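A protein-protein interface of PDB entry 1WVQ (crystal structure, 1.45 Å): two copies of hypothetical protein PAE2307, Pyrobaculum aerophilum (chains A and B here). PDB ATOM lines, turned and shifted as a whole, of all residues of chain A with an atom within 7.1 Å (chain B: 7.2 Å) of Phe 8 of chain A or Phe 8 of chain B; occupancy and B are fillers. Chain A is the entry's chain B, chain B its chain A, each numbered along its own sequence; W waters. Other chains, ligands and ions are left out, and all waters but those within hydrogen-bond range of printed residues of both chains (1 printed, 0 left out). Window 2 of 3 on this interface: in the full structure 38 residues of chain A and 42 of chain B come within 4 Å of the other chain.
Phe 8 of chain A touches Ile 6 of chain B, but with the chains exchanged Ile 6 of chain A does not touch Phe 8 of chain B (8.1 Å). Phe 8 of chain A touches its own counterpart, Phe 8 of chain B. Leu 10 of chain A touches Ile 6 of chain B, but with the chains exchanged Ile 6 of chain A does not touch Leu 10 of chain B (16.4 Å). Val 135 of chain B touches its own counterpart, Val 135 of chain A. 12 positions are printed for both chains.
Water W1 lies within hydrogen-bond range of the backbone carbonyl oxygen (O) of Val 135 of chain A and the backbone carbonyl oxygen (O) of Val 135 of chain B.
Of the 12 printed residues of chain B, 4 touch a printed residue of chain A. Along chain B the printed residues that touch a printed residue of chain A span positions 6 to 135. Among the printed residues, 5 pairs touch across the chains. Among the printed residues, no Asp or Glu carboxylate lies within 4 Å of a Lys or Arg side-chain nitrogen of the other chain.
The backbone carbonyl oxygen (O) of Val 135 of chain B lies close to the backbone carbonyl oxygen (O) of Val 135 of chain A (3.4 Å).
Of chain B, only Ile 6 (3.0 Å) and Phe 8 (3.9 Å) come within 4 Å of Phe 8 of chain A. Of chain A, only Phe 8 comes within 4 Å of Phe 8 of chain B. Of the printed residues of chain B, Ile 123 of chain A touches Ala 125 (3.8 Å). Of the printed residues of chain A, Val 135 of chain B touches Val 135. Printed residues of chain A within 4 Å of Ile 6 of chain B: Phe 8 and Leu 10. Of the printed residues of chain B, Val 135 of chain A touches Val 135. Of the printed residues of chain B, Leu 10 of chain A touches Ile 6. Ser 5 of chain B touches none of the printed residues of chain A. Val 124 of chain A touches none of the printed residues of chain B. The nearest residue of chain A that does not touch Phe 8 of chain B is Val 135 of chain A (5.3 Å). The nearest printed residue of chain B that does not touch Val 135 of chain A is Phe 8 of chain B (5.3 Å).
The backbone carbonyl oxygen (O) of Ile 123 of chain B is in hydrogen-bond range of the backbone NH (N) of Val 135 of chain B. N of Ala 125 of chain B lies within hydrogen-bond range of O of Gly 133 of chain B, 2.8 Å away. The backbone carbonyl oxygen of Ile 123 of chain A lies within hydrogen-bond range of the backbone NH of Val 135 of chain A, 2.8 Å away.
Among the printed residues, pairs that only touch across the chains: Phe 8 of chain A with Ile 6 of chain B (3.0 Å), Leu 10 of chain A with Ile 6 of chain B (3.5 Å), Ile 123 of chain A with Ala 125 of chain B (3.8 Å) and Phe 8 of chain A with Phe 8 of chain B (3.9 Å).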
ATOM      1  N   SER A   5     -27.446  -1.633   2.521  1.00  0.00           N
ATOM      2  CA  SER A   5     -28.085  -1.565   1.170  1.00  0.00           C
ATOM      3  C   SER A   5     -29.093  -2.698   1.066  1.00  0.00           C
ATOM      4  O   SER A   5     -29.541  -3.063  -0.025  1.00  0.00           O
ATOM      5  CB  SER A   5     -27.029  -1.720   0.076  1.00  0.00           C
ATOM      6  OG  SER A   5     -26.482  -3.031   0.068  1.00  0.00           O
ATOM      7  N   ILE A   6     -29.434  -3.236   2.230  1.00  0.00           N
ATOM      8  CA  ILE A   6     -30.365  -4.340   2.402  1.00  0.00           C
ATOM      9  C   ILE A   6     -30.981  -5.002   1.167  1.00  0.00           C
ATOM     10  O   ILE A   6     -30.517  -6.059   0.744  1.00  0.00           O
ATOM     11  CB  ILE A   6     -31.520  -3.948   3.363  1.00  0.00           C
ATOM     12  CG1 ILE A   6     -30.948  -3.475   4.699  1.00  0.00           C
ATOM     13  CG2 ILE A   6     -32.422  -5.155   3.609  1.00  0.00           C
ATOM     14  CD1 ILE A   6     -31.994  -3.173   5.763  1.00  0.00           C
ATOM     15  N   LYS A   7     -31.999  -4.387   0.574  1.00  0.00           N
ATOM     16  CA  LYS A   7     -32.679  -5.019  -0.552  1.00  0.00           C
ATOM     17  C   LYS A   7     -32.501  -4.393  -1.930  1.00  0.00           C
ATOM     18  O   LYS A   7     -32.607  -3.184  -2.093  1.00  0.00           O
ATOM     19  CB  LYS A   7     -34.170  -5.129  -0.218  1.00  0.00           C
ATOM     20  CG  LYS A   7     -34.424  -5.869   1.094  1.00  0.00           C
ATOM     21  CD  LYS A   7     -35.840  -5.681   1.623  1.00  0.00           C
ATOM     22  CE  LYS A   7     -36.061  -4.261   2.124  1.00  0.00           C
ATOM     23  NZ  LYS A   7     -35.032  -3.840   3.129  1.00  0.00           N
ATOM     24  N   PHE A   8     -32.228  -5.236  -2.918  1.00  0.00           N
ATOM     25  CA  PHE A   8     -32.055  -4.762  -4.287  1.00  0.00           C
ATOM     26  C   PHE A   8     -33.287  -5.145  -5.100  1.00  0.00           C
ATOM     27  O   PHE A   8     -33.843  -6.237  -4.933  1.00  0.00           O
ATOM     28  CB  PHE A   8     -30.812  -5.386  -4.918  1.00  0.00           C
ATOM     29  CG  PHE A   8     -29.521  -4.991  -4.257  1.00  0.00           C
ATOM     30  CD1 PHE A   8     -28.960  -3.736  -4.484  1.00  0.00           C
ATOM     31  CD2 PHE A   8     -28.860  -5.874  -3.410  1.00  0.00           C
ATOM     32  CE1 PHE A   8     -27.751  -3.375  -3.880  1.00  0.00           C
ATOM     33  CE2 PHE A   8     -27.657  -5.520  -2.803  1.00  0.00           C
ATOM     34  CZ  PHE A   8     -27.102  -4.269  -3.036  1.00  0.00           C
ATOM     35  N   GLU A   9     -33.711  -4.235  -5.969  1.00  0.00           N
ATOM     36  CA  GLU A   9     -34.881  -4.433  -6.815  1.00  0.00           C
ATOM     37  C   GLU A   9     -34.521  -4.115  -8.255  1.00  0.00           C
ATOM     38  O   GLU A   9     -33.616  -3.320  -8.515  1.00  0.00           O
ATOM     39  CB  GLU A   9     -36.019  -3.494  -6.391  1.00  0.00           C
ATOM     40  CG  GLU A   9     -36.744  -3.870  -5.116  1.00  0.00           C
ATOM     41  CD  GLU A   9     -37.791  -2.841  -4.722  1.00  0.00           C
ATOM     42  OE1 GLU A   9     -38.363  -2.191  -5.633  1.00  0.00           O
ATOM     43  OE2 GLU A   9     -38.051  -2.693  -3.503  1.00  0.00           O
ATOM     44  N   LEU A  10     -35.236  -4.732  -9.186  1.00  0.00           N
ATOM     45  CA  LEU A  10     -35.016  -4.485 -10.599  1.00  0.00           C
ATOM     46  C   LEU A  10     -36.258  -3.813 -11.165  1.00  0.00           C
ATOM     47  O   LEU A  10     -37.377  -4.307 -11.008  1.00  0.00           O
ATOM     48  CB  LEU A  10     -34.748  -5.792 -11.343  1.00  0.00           C
ATOM     49  CG  LEU A  10     -33.448  -6.511 -10.999  1.00  0.00           C
ATOM     50  CD1 LEU A  10     -33.359  -7.795 -11.801  1.00  0.00           C
ATOM     51  CD2 LEU A  10     -32.255  -5.607 -11.300  1.00  0.00           C
ATOM     52  N   ILE A 123     -31.414  -0.684 -11.354  1.00  0.00           N
ATOM     53  CA  ILE A 123     -31.225  -1.465 -10.144  1.00  0.00           C
ATOM     54  C   ILE A 123     -31.371  -0.483  -8.997  1.00  0.00           C
ATOM     55  O   ILE A 123     -30.632   0.498  -8.915  1.00  0.00           O
ATOM     56  CB  ILE A 123     -29.830  -2.115 -10.093  1.00  0.00           C
ATOM     57  CG1 ILE A 123     -29.614  -2.962 -11.348  1.00  0.00           C
ATOM     58  CG2 ILE A 123     -29.712  -2.997  -8.853  1.00  0.00           C
ATOM     59  CD1 ILE A 123     -28.242  -3.585 -11.442  1.00  0.00           C
ATOM     60  N   VAL A 124     -32.338  -0.741  -8.127  1.00  0.00           N
ATOM     61  CA  VAL A 124     -32.601   0.129  -6.992  1.00  0.00           C
ATOM     62  C   VAL A 124     -32.332  -0.587  -5.679  1.00  0.00           C
ATOM     63  O   VAL A 124     -32.641  -1.769  -5.532  1.00  0.00           O
ATOM     64  CB  VAL A 124     -34.071   0.609  -7.010  1.00  0.00           C
ATOM     65  CG1 VAL A 124     -34.376   1.448  -5.778  1.00  0.00           C
ATOM     66  CG2 VAL A 124     -34.333   1.406  -8.280  1.00  0.00           C
ATOM     67  N   ALA A 125     -31.737   0.128  -4.734  1.00  0.00           N
ATOM     68  CA  ALA A 125     -31.461  -0.439  -3.425  1.00  0.00           C
ATOM     69  C   ALA A 125     -32.417   0.199  -2.426  1.00  0.00           C
ATOM     70  O   ALA A 125     -32.623   1.409  -2.446  1.00  0.00           O
ATOM     71  CB  ALA A 125     -30.011  -0.154  -3.012  1.00  0.00           C
ATOM     72  N   GLU A 126     -33.028  -0.619  -1.575  1.00  0.00           N
ATOM     73  CA  GLU A 126     -33.922  -0.102  -0.543  1.00  0.00           C
ATOM     74  C   GLU A 126     -33.282  -0.505   0.775  1.00  0.00           C
ATOM     75  O   GLU A 126     -33.122  -1.696   1.062  1.00  0.00           O
ATOM     76  CB  GLU A 126     -35.330  -0.696  -0.652  1.00  0.00           C
ATOM     77  CG  GLU A 126     -36.264  -0.187   0.447  1.00  0.00           C
ATOM     78  CD  GLU A 126     -37.707  -0.590   0.234  1.00  0.00           C
ATOM     79  OE1 GLU A 126     -38.276  -0.247  -0.826  1.00  0.00           O
ATOM     80  OE2 GLU A 126     -38.276  -1.252   1.132  1.00  0.00           O
ATOM     81  N   GLY A 133     -32.381   4.188  -3.412  1.00  0.00           N
ATOM     82  CA  GLY A 133     -31.380   4.857  -4.227  1.00  0.00           C
ATOM     83  C   GLY A 133     -31.007   4.017  -5.435  1.00  0.00           C
ATOM     84  O   GLY A 133     -31.108   2.789  -5.397  1.00  0.00           O
ATOM     85  N   VAL A 135     -28.647   2.083  -7.803  1.00  0.00           N
ATOM     86  CA  VAL A 135     -27.345   1.436  -7.724  1.00  0.00           C
ATOM     87  C   VAL A 135     -26.673   1.465  -9.088  1.00  0.00           C
ATOM     88  O   VAL A 135     -25.474   1.734  -9.197  1.00  0.00           O
ATOM     89  CB  VAL A 135     -27.483  -0.023  -7.252  1.00  0.00           C
ATOM     90  CG1 VAL A 135     -26.180  -0.784  -7.490  1.00  0.00           C
ATOM     91  CG2 VAL A 135     -27.865  -0.047  -5.782  1.00  0.00           C
ATOM     92  N   SER B   5     -31.357 -14.416 -10.072  1.00  0.00           N
ATOM     93  CA  SER B   5     -31.619 -13.012  -9.645  1.00  0.00           C
ATOM     94  C   SER B   5     -30.449 -12.095 -10.005  1.00  0.00           C
ATOM     95  O   SER B   5     -29.800 -12.270 -11.037  1.00  0.00           O
ATOM     96  CB  SER B   5     -31.867 -12.965  -8.131  1.00  0.00           C
ATOM     97  OG  SER B   5     -30.795 -13.569  -7.423  1.00  0.00           O
ATOM     98  N   ILE B   6     -30.189 -11.111  -9.154  1.00  0.00           N
ATOM     99  CA  ILE B   6     -29.091 -10.180  -9.391  1.00  0.00           C
ATOM    100  C   ILE B   6     -27.770 -10.719  -8.840  1.00  0.00           C
ATOM    101  O   ILE B   6     -27.614 -10.908  -7.629  1.00  0.00           O
ATOM    102  CB  ILE B   6     -29.403  -8.817  -8.757  1.00  0.00           C
ATOM    103  CG1 ILE B   6     -29.821  -9.014  -7.305  1.00  0.00           C
ATOM    104  CG2 ILE B   6     -30.513  -8.125  -9.534  1.00  0.00           C
ATOM    105  CD1 ILE B   6     -30.436  -7.805  -6.670  1.00  0.00           C
ATOM    106  N   LYS B   7     -26.827 -10.975  -9.742  1.00  0.00           N
ATOM    107  CA  LYS B   7     -25.515 -11.497  -9.375  1.00  0.00           C
ATOM    108  C   LYS B   7     -24.418 -10.446  -9.516  1.00  0.00           C
ATOM    109  O   LYS B   7     -24.332  -9.766 -10.535  1.00  0.00           O
ATOM    110  CB  LYS B   7     -25.159 -12.701 -10.249  1.00  0.00           C
ATOM    111  CG  LYS B   7     -25.765 -14.027  -9.787  1.00  0.00           C
ATOM    112  CD  LYS B   7     -27.112 -14.344 -10.426  1.00  0.00           C
ATOM    113  CE  LYS B   7     -27.611 -15.711  -9.949  1.00  0.00           C
ATOM    114  NZ  LYS B   7     -28.832 -16.195 -10.659  1.00  0.00           N
ATOM    115  N   PHE B   8     -23.580 -10.324  -8.492  1.00  0.00           N
ATOM    116  CA  PHE B   8     -22.477  -9.366  -8.506  1.00  0.00           C
ATOM    117  C   PHE B   8     -21.152 -10.045  -8.828  1.00  0.00           C
ATOM    118  O   PHE B   8     -20.827 -11.097  -8.269  1.00  0.00           O
ATOM    119  CB  PHE B   8     -22.384  -8.657  -7.156  1.00  0.00           C
ATOM    120  CG  PHE B   8     -23.580  -7.821  -6.837  1.00  0.00           C
ATOM    121  CD1 PHE B   8     -23.863  -6.683  -7.582  1.00  0.00           C
ATOM    122  CD2 PHE B   8     -24.442  -8.180  -5.804  1.00  0.00           C
ATOM    123  CE1 PHE B   8     -24.979  -5.911  -7.303  1.00  0.00           C
ATOM    124  CE2 PHE B   8     -25.567  -7.413  -5.513  1.00  0.00           C
ATOM    125  CZ  PHE B   8     -25.840  -6.279  -6.264  1.00  0.00           C
ATOM    126  N   GLU B   9     -20.396  -9.428  -9.734  1.00  0.00           N
ATOM    127  CA  GLU B   9     -19.095  -9.916 -10.190  1.00  0.00           C
ATOM    128  C   GLU B   9     -18.045  -8.820 -10.001  1.00  0.00           C
ATOM    129  O   GLU B   9     -18.363  -7.630 -10.086  1.00  0.00           O
ATOM    130  CB  GLU B   9     -19.140 -10.229 -11.688  1.00  0.00           C
ATOM    131  CG  GLU B   9     -19.320 -11.674 -12.101  1.00  0.00           C
ATOM    132  CD  GLU B   9     -19.332 -11.823 -13.621  1.00  0.00           C
ATOM    133  OE1 GLU B   9     -18.396 -11.317 -14.288  1.00  0.00           O
ATOM    134  OE2 GLU B   9     -20.270 -12.447 -14.156  1.00  0.00           O
ATOM    135  N   LEU B  10     -16.801  -9.228  -9.758  1.00  0.00           N
ATOM    136  CA  LEU B  10     -15.693  -8.285  -9.608  1.00  0.00           C
ATOM    137  C   LEU B  10     -14.724  -8.476 -10.770  1.00  0.00           C
ATOM    138  O   LEU B  10     -14.305  -9.596 -11.059  1.00  0.00           O
ATOM    139  CB  LEU B  10     -14.941  -8.502  -8.289  1.00  0.00           C
ATOM    140  CG  LEU B  10     -15.608  -8.103  -6.975  1.00  0.00           C
ATOM    141  CD1 LEU B  10     -14.608  -8.284  -5.835  1.00  0.00           C
ATOM    142  CD2 LEU B  10     -16.064  -6.658  -7.042  1.00  0.00           C
ATOM    143  N   ILE B 123     -17.161  -3.370 -10.272  1.00  0.00           N
ATOM    144  CA  ILE B 123     -18.224  -4.237  -9.781  1.00  0.00           C
ATOM    145  C   ILE B 123     -19.314  -4.274 -10.839  1.00  0.00           C
ATOM    146  O   ILE B 123     -19.871  -3.241 -11.211  1.00  0.00           O
ATOM    147  CB  ILE B 123     -18.832  -3.721  -8.463  1.00  0.00           C
ATOM    148  CG1 ILE B 123     -17.732  -3.529  -7.414  1.00  0.00           C
ATOM    149  CG2 ILE B 123     -19.877  -4.724  -7.947  1.00  0.00           C
ATOM    150  CD1 ILE B 123     -18.217  -2.881  -6.140  1.00  0.00           C
ATOM    151  N   VAL B 124     -19.618  -5.472 -11.319  1.00  0.00           N
ATOM    152  CA  VAL B 124     -20.632  -5.643 -12.348  1.00  0.00           C
ATOM    153  C   VAL B 124     -21.811  -6.467 -11.851  1.00  0.00           C
ATOM    154  O   VAL B 124     -21.646  -7.408 -11.072  1.00  0.00           O
ATOM    155  CB  VAL B 124     -20.020  -6.327 -13.592  1.00  0.00           C
ATOM    156  CG1 VAL B 124     -21.071  -6.519 -14.677  1.00  0.00           C
ATOM    157  CG2 VAL B 124     -18.868  -5.486 -14.114  1.00  0.00           C
ATOM    158  N   ALA B 125     -23.003  -6.090 -12.294  1.00  0.00           N
ATOM    159  CA  ALA B 125     -24.205  -6.812 -11.929  1.00  0.00           C
ATOM    160  C   ALA B 125     -24.791  -7.457 -13.175  1.00  0.00           C
ATOM    161  O   ALA B 125     -24.922  -6.817 -14.217  1.00  0.00           O
ATOM    162  CB  ALA B 125     -25.225  -5.867 -11.307  1.00  0.00           C
ATOM    163  N   GLU B 126     -25.112  -8.739 -13.066  1.00  0.00           N
ATOM    164  CA  GLU B 126     -25.736  -9.457 -14.165  1.00  0.00           C
ATOM    165  C   GLU B 126     -27.126  -9.792 -13.634  1.00  0.00           C
ATOM    166  O   GLU B 126     -27.261 -10.411 -12.574  1.00  0.00           O
ATOM    167  CB  GLU B 126     -24.965 -10.732 -14.512  1.00  0.00           C
ATOM    168  CG  GLU B 126     -25.489 -11.397 -15.778  1.00  0.00           C
ATOM    169  CD  GLU B 126     -24.607 -12.525 -16.283  1.00  0.00           C
ATOM    170  OE1 GLU B 126     -23.394 -12.300 -16.483  1.00  0.00           O
ATOM    171  OE2 GLU B 126     -25.136 -13.639 -16.492  1.00  0.00           O
ATOM    172  N   GLY B 133     -24.532  -4.582 -16.049  1.00  0.00           N
ATOM    173  CA  GLY B 133     -24.353  -3.159 -15.838  1.00  0.00           C
ATOM    174  C   GLY B 133     -23.326  -2.908 -14.750  1.00  0.00           C
ATOM    175  O   GLY B 133     -23.094  -3.764 -13.893  1.00  0.00           O
ATOM    176  N   VAL B 135     -22.050  -1.457 -11.393  1.00  0.00           N
ATOM    177  CA  VAL B 135     -22.568  -1.019 -10.101  1.00  0.00           C
ATOM    178  C   VAL B 135     -21.663   0.070  -9.539  1.00  0.00           C
ATOM    179  O   VAL B 135     -22.137   1.063  -8.987  1.00  0.00           O
ATOM    180  CB  VAL B 135     -22.623  -2.191  -9.089  1.00  0.00           C
ATOM    181  CG1 VAL B 135     -22.937  -1.667  -7.688  1.00  0.00           C
ATOM    182  CG2 VAL B 135     -23.670  -3.201  -9.526  1.00  0.00           C
HETATM  183  O   HOH W   1     -23.730   2.541 -11.050  1.00  0.00           O
